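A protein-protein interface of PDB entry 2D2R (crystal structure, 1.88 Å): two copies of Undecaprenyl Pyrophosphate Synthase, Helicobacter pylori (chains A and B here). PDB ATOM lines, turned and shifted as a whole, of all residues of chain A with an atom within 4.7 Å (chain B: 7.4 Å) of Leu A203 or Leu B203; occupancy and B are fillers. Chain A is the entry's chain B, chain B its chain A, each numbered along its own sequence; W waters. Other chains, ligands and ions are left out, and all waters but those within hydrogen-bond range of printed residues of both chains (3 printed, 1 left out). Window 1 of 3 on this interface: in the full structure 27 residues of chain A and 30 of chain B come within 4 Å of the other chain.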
ATOM      1  N   SER A 145       8.414 -15.717  25.533  1.00  0.00           N
ATOM      2  CA  SER A 145       9.174 -16.579  24.596  1.00  0.00           C
ATOM      3  C   SER A 145      10.109 -17.543  25.247  1.00  0.00           C
ATOM      4  O   SER A 145      10.222 -18.695  24.807  1.00  0.00           O
ATOM      5  CB  SER A 145      10.106 -15.788  23.645  1.00  0.00           C
ATOM      6  OG  SER A 145       9.368 -15.014  22.810  1.00  0.00           O
ATOM      7  N   LEU A 198      11.253  -5.792  22.589  1.00  0.00           N
ATOM      8  CA  LEU A 198      10.438  -6.962  22.147  1.00  0.00           C
ATOM      9  C   LEU A 198       9.641  -7.592  23.269  1.00  0.00           C
ATOM     10  O   LEU A 198       8.681  -8.340  23.047  1.00  0.00           O
ATOM     11  CB  LEU A 198      11.350  -8.042  21.565  1.00  0.00           C
ATOM     12  CG  LEU A 198      12.372  -7.491  20.563  1.00  0.00           C
ATOM     13  CD1 LEU A 198      13.636  -8.463  20.343  1.00  0.00           C
ATOM     14  CD2 LEU A 198      11.560  -7.295  19.275  1.00  0.00           C
ATOM     15  N   ASN A 200      10.102 -10.094  25.293  1.00  0.00           N
ATOM     16  CA  ASN A 200       9.980 -11.535  25.388  1.00  0.00           C
ATOM     17  C   ASN A 200       8.754 -12.091  24.658  1.00  0.00           C
ATOM     18  O   ASN A 200       8.082 -12.993  25.119  1.00  0.00           O
ATOM     19  CB  ASN A 200       9.987 -11.853  26.926  1.00  0.00           C
ATOM     20  CG  ASN A 200      10.110 -13.314  27.211  1.00  0.00           C
ATOM     21  OD1 ASN A 200      10.782 -14.039  26.467  1.00  0.00           O
ATOM     22  ND2 ASN A 200       9.475 -13.781  28.310  1.00  0.00           N
ATOM     23  N   PHE A 201       8.506 -11.541  23.477  1.00  0.00           N
ATOM     24  CA  PHE A 201       7.352 -11.936  22.689  1.00  0.00           C
ATOM     25  C   PHE A 201       7.787 -12.431  21.322  1.00  0.00           C
ATOM     26  O   PHE A 201       8.397 -11.675  20.548  1.00  0.00           O
ATOM     27  CB  PHE A 201       6.456 -10.707  22.561  1.00  0.00           C
ATOM     28  CG  PHE A 201       5.229 -10.927  21.740  1.00  0.00           C
ATOM     29  CD1 PHE A 201       4.287 -11.885  22.076  1.00  0.00           C
ATOM     30  CD2 PHE A 201       5.016 -10.126  20.612  1.00  0.00           C
ATOM     31  CE1 PHE A 201       3.135 -12.020  21.257  1.00  0.00           C
ATOM     32  CE2 PHE A 201       3.873 -10.249  19.813  1.00  0.00           C
ATOM     33  CZ  PHE A 201       2.944 -11.198  20.138  1.00  0.00           C
ATOM     34  N   LEU A 202       7.499 -13.699  21.031  1.00  0.00           N
ATOM     35  CA  LEU A 202       7.817 -14.237  19.676  1.00  0.00           C
ATOM     36  C   LEU A 202       9.228 -13.951  19.188  1.00  0.00           C
ATOM     37  O   LEU A 202       9.431 -13.702  18.012  1.00  0.00           O
ATOM     38  CB  LEU A 202       6.809 -13.713  18.613  1.00  0.00           C
ATOM     39  CG  LEU A 202       5.312 -14.006  18.896  1.00  0.00           C
ATOM     40  CD1 LEU A 202       4.418 -13.400  17.804  1.00  0.00           C
ATOM     41  CD2 LEU A 202       5.064 -15.539  18.997  1.00  0.00           C
ATOM     42  N   LEU A 203      10.191 -14.108  20.082  1.00  0.00           N
ATOM     43  CA  LEU A 203      11.582 -13.849  19.724  1.00  0.00           C
ATOM     44  C   LEU A 203      12.038 -14.766  18.568  1.00  0.00           C
ATOM     45  O   LEU A 203      12.637 -14.302  17.606  1.00  0.00           O
ATOM     46  CB  LEU A 203      12.477 -14.075  20.953  1.00  0.00           C
ATOM     47  CG  LEU A 203      12.096 -13.251  22.194  1.00  0.00           C
ATOM     48  CD1 LEU A 203      12.947 -13.699  23.428  1.00  0.00           C
ATOM     49  CD2 LEU A 203      12.298 -11.777  21.893  1.00  0.00           C
ATOM     50  N   TRP A 204      11.783 -16.074  18.683  1.00  0.00           N
ATOM     51  CA  TRP A 204      12.201 -17.040  17.665  1.00  0.00           C
ATOM     52  C   TRP A 204      11.503 -16.852  16.367  1.00  0.00           C
ATOM     53  O   TRP A 204      12.100 -16.858  15.282  1.00  0.00           O
ATOM     54  CB  TRP A 204      11.887 -18.444  18.188  1.00  0.00           C
ATOM     55  CG  TRP A 204      12.141 -19.557  17.260  1.00  0.00           C
ATOM     56  CD1 TRP A 204      11.356 -19.967  16.224  1.00  0.00           C
ATOM     57  CD2 TRP A 204      13.261 -20.468  17.315  1.00  0.00           C
ATOM     58  NE1 TRP A 204      11.913 -21.109  15.614  1.00  0.00           N
ATOM     59  CE2 TRP A 204      13.072 -21.432  16.281  1.00  0.00           C
ATOM     60  CE3 TRP A 204      14.415 -20.557  18.153  1.00  0.00           C
ATOM     61  CZ2 TRP A 204      13.977 -22.481  16.061  1.00  0.00           C
ATOM     62  CZ3 TRP A 204      15.315 -21.583  17.940  1.00  0.00           C
ATOM     63  CH2 TRP A 204      15.091 -22.544  16.896  1.00  0.00           C
ATOM     64  N   GLN A 205      10.183 -16.705  16.483  1.00  0.00           N
ATOM     65  CA  GLN A 205       9.319 -16.536  15.321  1.00  0.00           C
ATOM     66  C   GLN A 205       9.472 -15.205  14.593  1.00  0.00           C
ATOM     67  O   GLN A 205       9.038 -15.082  13.413  1.00  0.00           O
ATOM     68  CB  GLN A 205       7.846 -16.678  15.755  1.00  0.00           C
ATOM     69  CG  GLN A 205       7.501 -18.016  16.451  1.00  0.00           C
ATOM     70  CD  GLN A 205       7.649 -17.934  17.962  1.00  0.00           C
ATOM     71  OE1 GLN A 205       8.425 -17.116  18.501  1.00  0.00           O
ATOM     72  NE2 GLN A 205       6.921 -18.807  18.666  1.00  0.00           N
ATOM     73  N   SER A 206      10.052 -14.209  15.264  1.00  0.00           N
ATOM     74  CA  SER A 206      10.236 -12.880  14.638  1.00  0.00           C
ATOM     75  C   SER A 206      11.671 -12.676  14.202  1.00  0.00           C
ATOM     76  O   SER A 206      12.078 -11.547  13.999  1.00  0.00           O
ATOM     77  CB  SER A 206       9.882 -11.780  15.651  1.00  0.00           C
ATOM     78  OG  SER A 206       8.553 -11.990  16.143  1.00  0.00           O
ATOM     79  N   SER A 207      12.449 -13.762  14.111  1.00  0.00           N
ATOM     80  CA  SER A 207      13.876 -13.632  13.755  1.00  0.00           C
ATOM     81  C   SER A 207      14.228 -12.694  12.575  1.00  0.00           C
ATOM     82  O   SER A 207      15.312 -12.003  12.595  1.00  0.00           O
ATOM     83  CB  SER A 207      14.454 -15.017  13.449  1.00  0.00           C
ATOM     84  OG  SER A 207      15.863 -14.815  13.396  1.00  0.00           O
ATOM     85  N   TYR B 143      27.596 -16.816  13.109  1.00  0.00           N
ATOM     86  CA  TYR B 143      26.568 -16.809  14.161  1.00  0.00           C
ATOM     87  C   TYR B 143      25.124 -16.683  13.713  1.00  0.00           C
ATOM     88  O   TYR B 143      24.798 -15.875  12.836  1.00  0.00           O
ATOM     89  CB  TYR B 143      26.837 -15.646  15.124  1.00  0.00           C
ATOM     90  CG  TYR B 143      25.814 -15.566  16.242  1.00  0.00           C
ATOM     91  CD1 TYR B 143      25.987 -16.280  17.442  1.00  0.00           C
ATOM     92  CD2 TYR B 143      24.614 -14.871  16.056  1.00  0.00           C
ATOM     93  CE1 TYR B 143      24.952 -16.296  18.444  1.00  0.00           C
ATOM     94  CE2 TYR B 143      23.592 -14.887  17.032  1.00  0.00           C
ATOM     95  CZ  TYR B 143      23.749 -15.589  18.211  1.00  0.00           C
ATOM     96  OH  TYR B 143      22.680 -15.603  19.132  1.00  0.00           O
ATOM     97  N   GLY B 144      24.256 -17.462  14.376  1.00  0.00           N
ATOM     98  CA  GLY B 144      22.834 -17.365  14.099  1.00  0.00           C
ATOM     99  C   GLY B 144      22.161 -17.720  15.412  1.00  0.00           C
ATOM    100  O   GLY B 144      22.570 -18.679  16.034  1.00  0.00           O
ATOM    101  N   SER B 145      21.145 -16.968  15.824  1.00  0.00           N
ATOM    102  CA  SER B 145      20.455 -17.244  17.083  1.00  0.00           C
ATOM    103  C   SER B 145      19.725 -18.560  17.107  1.00  0.00           C
ATOM    104  O   SER B 145      19.819 -19.311  18.073  1.00  0.00           O
ATOM    105  CB  SER B 145      19.532 -16.033  17.363  1.00  0.00           C
ATOM    106  OG  SER B 145      19.073 -16.063  18.649  1.00  0.00           O
ATOM    107  N   LYS B 146      18.968 -18.885  16.055  1.00  0.00           N
ATOM    108  CA  LYS B 146      18.306 -20.161  16.073  1.00  0.00           C
ATOM    109  C   LYS B 146      19.310 -21.280  16.163  1.00  0.00           C
ATOM    110  O   LYS B 146      19.080 -22.265  16.843  1.00  0.00           O
ATOM    111  CB  LYS B 146      17.435 -20.360  14.840  1.00  0.00           C
ATOM    112  CG  LYS B 146      16.226 -19.509  14.885  1.00  0.00           C
ATOM    113  CD  LYS B 146      15.331 -19.847  13.669  1.00  0.00           C
ATOM    114  CE  LYS B 146      13.999 -19.034  13.765  1.00  0.00           C
ATOM    115  NZ  LYS B 146      13.088 -19.476  12.681  1.00  0.00           N
ATOM    116  N   GLU B 148      22.335 -21.071  17.532  1.00  0.00           N
ATOM    117  CA  GLU B 148      22.882 -21.084  18.890  1.00  0.00           C
ATOM    118  C   GLU B 148      21.935 -21.826  19.847  1.00  0.00           C
ATOM    119  O   GLU B 148      22.362 -22.632  20.666  1.00  0.00           O
ATOM    120  CB  GLU B 148      23.121 -19.674  19.421  1.00  0.00           C
ATOM    121  CG  GLU B 148      23.749 -19.616  20.843  1.00  0.00           C
ATOM    122  CD  GLU B 148      23.728 -18.198  21.447  1.00  0.00           C
ATOM    123  OE1 GLU B 148      22.899 -17.336  21.005  1.00  0.00           O
ATOM    124  OE2 GLU B 148      24.535 -17.950  22.364  1.00  0.00           O
ATOM    125  N   LEU B 149      20.633 -21.560  19.744  1.00  0.00           N
ATOM    126  CA  LEU B 149      19.682 -22.233  20.610  1.00  0.00           C
ATOM    127  C   LEU B 149      19.630 -23.726  20.327  1.00  0.00           C
ATOM    128  O   LEU B 149      19.445 -24.553  21.255  1.00  0.00           O
ATOM    129  CB  LEU B 149      18.288 -21.590  20.471  1.00  0.00           C
ATOM    130  CG  LEU B 149      18.236 -20.255  21.245  1.00  0.00           C
ATOM    131  CD1 LEU B 149      17.109 -19.321  20.685  1.00  0.00           C
ATOM    132  CD2 LEU B 149      18.007 -20.568  22.768  1.00  0.00           C
ATOM    133  N   GLU B 185      22.736  -9.877  30.149  1.00  0.00           N
ATOM    134  CA  GLU B 185      21.819  -9.821  29.033  1.00  0.00           C
ATOM    135  C   GLU B 185      22.070  -8.521  28.284  1.00  0.00           C
ATOM    136  O   GLU B 185      22.754  -7.583  28.768  1.00  0.00           O
ATOM    137  CB  GLU B 185      20.344  -9.866  29.510  1.00  0.00           C
ATOM    138  CG  GLU B 185      19.924 -11.204  30.140  1.00  0.00           C
ATOM    139  CD  GLU B 185      20.037 -12.415  29.176  1.00  0.00           C
ATOM    140  OE1 GLU B 185      19.165 -12.596  28.292  1.00  0.00           O
ATOM    141  OE2 GLU B 185      20.987 -13.208  29.330  1.00  0.00           O
ATOM    142  N   LEU B 189      20.266  -2.926  21.928  1.00  0.00           N
ATOM    143  CA  LEU B 189      20.649  -3.597  20.673  1.00  0.00           C
ATOM    144  C   LEU B 189      20.509  -2.547  19.590  1.00  0.00           C
ATOM    145  O   LEU B 189      19.432  -1.997  19.357  1.00  0.00           O
ATOM    146  CB  LEU B 189      19.716  -4.801  20.382  1.00  0.00           C
ATOM    147  CG  LEU B 189      19.936  -5.426  19.002  1.00  0.00           C
ATOM    148  CD1 LEU B 189      21.390  -5.953  18.906  1.00  0.00           C
ATOM    149  CD2 LEU B 189      18.988  -6.562  18.793  1.00  0.00           C
ATOM    150  N   LEU B 198      15.777  -7.911  13.335  1.00  0.00           N
ATOM    151  CA  LEU B 198      16.797  -8.411  14.289  1.00  0.00           C
ATOM    152  C   LEU B 198      17.820  -9.285  13.564  1.00  0.00           C
ATOM    153  O   LEU B 198      18.947  -9.491  14.041  1.00  0.00           O
ATOM    154  CB  LEU B 198      16.178  -9.300  15.357  1.00  0.00           C
ATOM    155  CG  LEU B 198      15.060  -8.580  16.061  1.00  0.00           C
ATOM    156  CD1 LEU B 198      14.214  -9.642  16.831  1.00  0.00           C
ATOM    157  CD2 LEU B 198      15.663  -7.575  16.997  1.00  0.00           C
ATOM    158  N   SER B 199      17.386  -9.830  12.438  1.00  0.00           N
ATOM    159  CA  SER B 199      18.235 -10.707  11.667  1.00  0.00           C
ATOM    160  C   SER B 199      18.858 -11.867  12.422  1.00  0.00           C
ATOM    161  O   SER B 199      20.068 -12.113  12.290  1.00  0.00           O
ATOM    162  CB  SER B 199      19.320  -9.868  10.967  1.00  0.00           C
ATOM    163  OG  SER B 199      18.689  -9.188   9.882  1.00  0.00           O
ATOM    164  N   ASN B 200      18.052 -12.583  13.202  1.00  0.00           N
ATOM    165  CA  ASN B 200      18.518 -13.814  13.886  1.00  0.00           C
ATOM    166  C   ASN B 200      19.778 -13.588  14.751  1.00  0.00           C
ATOM    167  O   ASN B 200      20.677 -14.401  14.786  1.00  0.00           O
ATOM    168  CB  ASN B 200      18.775 -14.829  12.775  1.00  0.00           C
ATOM    169  CG  ASN B 200      18.882 -16.239  13.269  1.00  0.00           C
ATOM    170  OD1 ASN B 200      18.313 -16.620  14.285  1.00  0.00           O
ATOM    171  ND2 ASN B 200      19.674 -17.043  12.548  1.00  0.00           N
ATOM    172  N   PHE B 201      19.824 -12.447  15.406  1.00  0.00           N
ATOM    173  CA  PHE B 201      20.932 -12.063  16.256  1.00  0.00           C
ATOM    174  C   PHE B 201      20.525 -11.860  17.704  1.00  0.00           C
ATOM    175  O   PHE B 201      19.703 -10.968  18.038  1.00  0.00           O
ATOM    176  CB  PHE B 201      21.528 -10.769  15.683  1.00  0.00           C
ATOM    177  CG  PHE B 201      22.718 -10.200  16.454  1.00  0.00           C
ATOM    178  CD1 PHE B 201      23.878 -10.942  16.629  1.00  0.00           C
ATOM    179  CD2 PHE B 201      22.689  -8.894  16.944  1.00  0.00           C
ATOM    180  CE1 PHE B 201      25.026 -10.373  17.289  1.00  0.00           C
ATOM    181  CE2 PHE B 201      23.805  -8.322  17.596  1.00  0.00           C
ATOM    182  CZ  PHE B 201      24.977  -9.069  17.759  1.00  0.00           C
ATOM    183  N   LEU B 202      21.108 -12.676  18.575  1.00  0.00           N
ATOM    184  CA  LEU B 202      20.916 -12.560  20.024  1.00  0.00           C
ATOM    185  C   LEU B 202      19.432 -12.397  20.373  1.00  0.00           C
ATOM    186  O   LEU B 202      19.071 -11.540  21.169  1.00  0.00           O
ATOM    187  CB  LEU B 202      21.687 -11.333  20.552  1.00  0.00           C
ATOM    188  CG  LEU B 202      23.229 -11.370  20.363  1.00  0.00           C
ATOM    189  CD1 LEU B 202      23.886 -10.083  20.991  1.00  0.00           C
ATOM    190  CD2 LEU B 202      23.729 -12.608  21.024  1.00  0.00           C
ATOM    191  N   LEU B 203      18.600 -13.259  19.821  1.00  0.00           N
ATOM    192  CA  LEU B 203      17.137 -13.160  20.060  1.00  0.00           C
ATOM    193  C   LEU B 203      16.810 -13.372  21.548  1.00  0.00           C
ATOM    194  O   LEU B 203      16.118 -12.579  22.190  1.00  0.00           O
ATOM    195  CB  LEU B 203      16.437 -14.169  19.178  1.00  0.00           C
ATOM    196  CG  LEU B 203      16.700 -14.025  17.664  1.00  0.00           C
ATOM    197  CD1 LEU B 203      16.055 -15.193  16.852  1.00  0.00           C
ATOM    198  CD2 LEU B 203      16.069 -12.757  17.198  1.00  0.00           C
ATOM    199  N   TRP B 204      17.370 -14.425  22.110  1.00  0.00           N
ATOM    200  CA  TRP B 204      17.159 -14.748  23.502  1.00  0.00           C
ATOM    201  C   TRP B 204      17.736 -13.702  24.414  1.00  0.00           C
ATOM    202  O   TRP B 204      17.055 -13.256  25.322  1.00  0.00           O
ATOM    203  CB  TRP B 204      17.777 -16.112  23.797  1.00  0.00           C
ATOM    204  CG  TRP B 204      17.689 -16.546  25.248  1.00  0.00           C
ATOM    205  CD1 TRP B 204      18.458 -16.082  26.324  1.00  0.00           C
ATOM    206  CD2 TRP B 204      16.865 -17.578  25.771  1.00  0.00           C
ATOM    207  NE1 TRP B 204      18.137 -16.783  27.457  1.00  0.00           N
ATOM    208  CE2 TRP B 204      17.175 -17.713  27.142  1.00  0.00           C
ATOM    209  CE3 TRP B 204      15.892 -18.423  25.206  1.00  0.00           C
ATOM    210  CZ2 TRP B 204      16.543 -18.654  27.958  1.00  0.00           C
ATOM    211  CZ3 TRP B 204      15.276 -19.345  26.002  1.00  0.00           C
ATOM    212  CH2 TRP B 204      15.602 -19.462  27.373  1.00  0.00           C
ATOM    213  N   GLN B 205      18.970 -13.281  24.148  1.00  0.00           N
ATOM    214  CA  GLN B 205      19.647 -12.337  25.022  1.00  0.00           C
ATOM    215  C   GLN B 205      19.145 -10.912  24.980  1.00  0.00           C
ATOM    216  O   GLN B 205      19.412 -10.168  25.869  1.00  0.00           O
ATOM    217  CB  GLN B 205      21.185 -12.342  24.741  1.00  0.00           C
ATOM    218  CG  GLN B 205      21.753 -13.786  24.837  1.00  0.00           C
ATOM    219  CD  GLN B 205      21.714 -14.637  23.541  1.00  0.00           C
ATOM    220  OE1 GLN B 205      20.862 -14.450  22.663  1.00  0.00           O
ATOM    221  NE2 GLN B 205      22.639 -15.649  23.455  1.00  0.00           N
ATOM    222  N   SER B 206      18.420 -10.559  23.927  1.00  0.00           N
ATOM    223  CA  SER B 206      17.908  -9.206  23.758  1.00  0.00           C
ATOM    224  C   SER B 206      16.389  -9.181  24.061  1.00  0.00           C
ATOM    225  O   SER B 206      15.736  -8.254  23.639  1.00  0.00           O
ATOM    226  CB  SER B 206      18.160  -8.764  22.291  1.00  0.00           C
ATOM    227  OG  SER B 206      19.547  -8.955  21.912  1.00  0.00           O
ATOM    228  N   SER B 207      15.854 -10.156  24.798  1.00  0.00           N
ATOM    229  CA  SER B 207      14.397 -10.189  25.026  1.00  0.00           C
ATOM    230  C   SER B 207      13.842  -8.896  25.626  1.00  0.00           C
ATOM    231  O   SER B 207      12.650  -8.559  25.435  1.00  0.00           O
ATOM    232  CB  SER B 207      14.017 -11.363  25.941  1.00  0.00           C
ATOM    233  OG  SER B 207      14.666 -11.189  27.199  1.00  0.00           O
ATOM    234  N   TYR B 208      14.690  -8.181  26.359  1.00  0.00           N
ATOM    235  CA  TYR B 208      14.241  -6.915  26.952  1.00  0.00           C
ATOM    236  C   TYR B 208      15.126  -5.727  26.655  1.00  0.00           C
ATOM    237  O   TYR B 208      15.034  -4.640  27.276  1.00  0.00           O
ATOM    238  CB  TYR B 208      14.018  -7.075  28.465  1.00  0.00           C
ATOM    239  CG  TYR B 208      12.761  -7.890  28.825  1.00  0.00           C
ATOM    240  CD1 TYR B 208      11.477  -7.302  28.851  1.00  0.00           C
ATOM    241  CD2 TYR B 208      12.871  -9.242  29.175  1.00  0.00           C
ATOM    242  CE1 TYR B 208      10.330  -8.065  29.217  1.00  0.00           C
ATOM    243  CE2 TYR B 208      11.746  -9.991  29.543  1.00  0.00           C
ATOM    244  CZ  TYR B 208      10.498  -9.397  29.552  1.00  0.00           C
ATOM    245  OH  TYR B 208       9.416 -10.210  29.878  1.00  0.00           O
HETATM  246  O   HOH W   1      12.644 -21.986  12.545  1.00  0.00           O
HETATM  247  O   HOH W   2      13.395  -8.910  13.227  1.00  0.00           O
HETATM  248  O   HOH W   3      13.893  -6.200  23.211  1.00  0.00           O
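Leu A203 touches just these residues of chain B: Leu B203 and Ser B207.
Printed residues of chain A within 4 Å of Leu B203: Leu A203 (3.6 Å) and Ser A207 (3.5 Å).
Printed residues of chain A within 4 Å of Ser B199: Ser A207.
Printed residues of chain A within 4 Å of Asn B200: Ser A207 (2.9 Å).
Of the printed residues of chain A, Leu B149 touches Trp A204.
Of the printed residues of chain B, Leu A198 touches Leu B198 (3.7 Å), Ser B206 (3.9 Å) and Ser B207 (3.8 Å).
Of the printed residues of chain B, Trp A204 touches Lys B146 (3.3 Å) and Leu B149 (3.9 Å).
Leu A202 touches none of the printed residues of chain B.
Gly B144 touches none of the printed residues of chain A.
The nearest residue of chain B that does not touch Leu A203 is Trp B204 (4.3 Å).
The nearest printed residue of chain A that does not touch Tyr B208 is Leu A198 (5.4 Å).
Printed residues of chain B that touch a printed residue of chain A: Lys B146, Leu B149, Leu B198, Ser B199, Asn B200, Leu B203, Ser B206, Ser B207 and Tyr B208.
Hydrophobic or aromatic side chains of chain B that line the printed part of chain A: Leu B149, Leu B198, Leu B203 and Tyr B208.
Among the printed residues, 13 pairs touch across the chains.
Among the printed residues, no Asp or Glu carboxylate lies within 4 Å of a Lys or Arg side-chain nitrogen of the other chain.
The backbone NH (N) of Ser A145 is in hydrogen-bond range of the backbone carbonyl oxygen (O) of Asn A200, at 2.8 Å.
The backbone NH (N) of Leu B203 is in hydrogen-bond range of the side-chain hydroxyl (OG) of Ser B145 (3.1 Å).
OG of Ser A145 is in hydrogen-bond range of N of Leu A203 (3.0 Å).
The side-chain amide oxygen of Asn B200 sits at hydrogen-bond distance from the backbone NH of Lys B146.
O of Leu B202 is in hydrogen-bond range of OG of Ser B206.
The backbone NH (N) of Ser B145 lies within hydrogen-bond range of the backbone carbonyl oxygen (O) of Asn B200 (2.8 Å).
Leu A198 touches its own counterpart, Leu B198.
Leu A198 touches Ser B206, but with the chains exchanged Ser A206 does not touch Leu B198 (4.03 Å).
Leu A198 touches Ser B207, and with the chains exchanged Ser A207 touches Leu B198.
Leu B203 touches its own counterpart, Leu A203.
Of the 13 pairs that touch across the chains among the printed residues, 8 have their exchanged pair printed and touching as well.
O of Ser A207 lies within hydrogen-bond range of N of Asn B200 (2.9 Å).
The backbone NH (N) of Ser B199 is in hydrogen-bond range of the backbone carbonyl oxygen (O) of Ser A207 (3.0 Å).
O of Ser B207 is in hydrogen-bond range of N of Asn A200 (3.0 Å).
Water W1 bridges the side-chain amino group (NZ) of Lys B146 (2.6 Å) and the indole nitrogen (NE1) of Trp A204 (3.3 Å).
Water W2 bridges N of Leu B198 (2.6 Å) and O of Ser A206 (3.0 Å).
Water W3 lies within hydrogen-bond range of N of Leu A198, O of Ser B206 and O of Ser B207.
Leu A198 touches Leu B198.
Leu A198 touches Ser B206 (CD1 to O, 3.9 Å).
Ser B207 touches Leu A198.
Asn A200 touches Tyr B208.
Leu A203 touches Leu B203 (CD1 to O, 3.6 Å).
CD1 of Leu A203 touches CB of Ser B207, 3.6 Å away.
Lys B146 touches Trp A204 (CE to O, 3.3 Å).
Trp A204 touches Leu B149 (CE3 to CD1, 3.9 Å).
Ser A207 touches Leu B198 (O to C, 3.8 Å).
OG of Ser A207 touches CD1 of Leu B203, 3.5 Å away.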
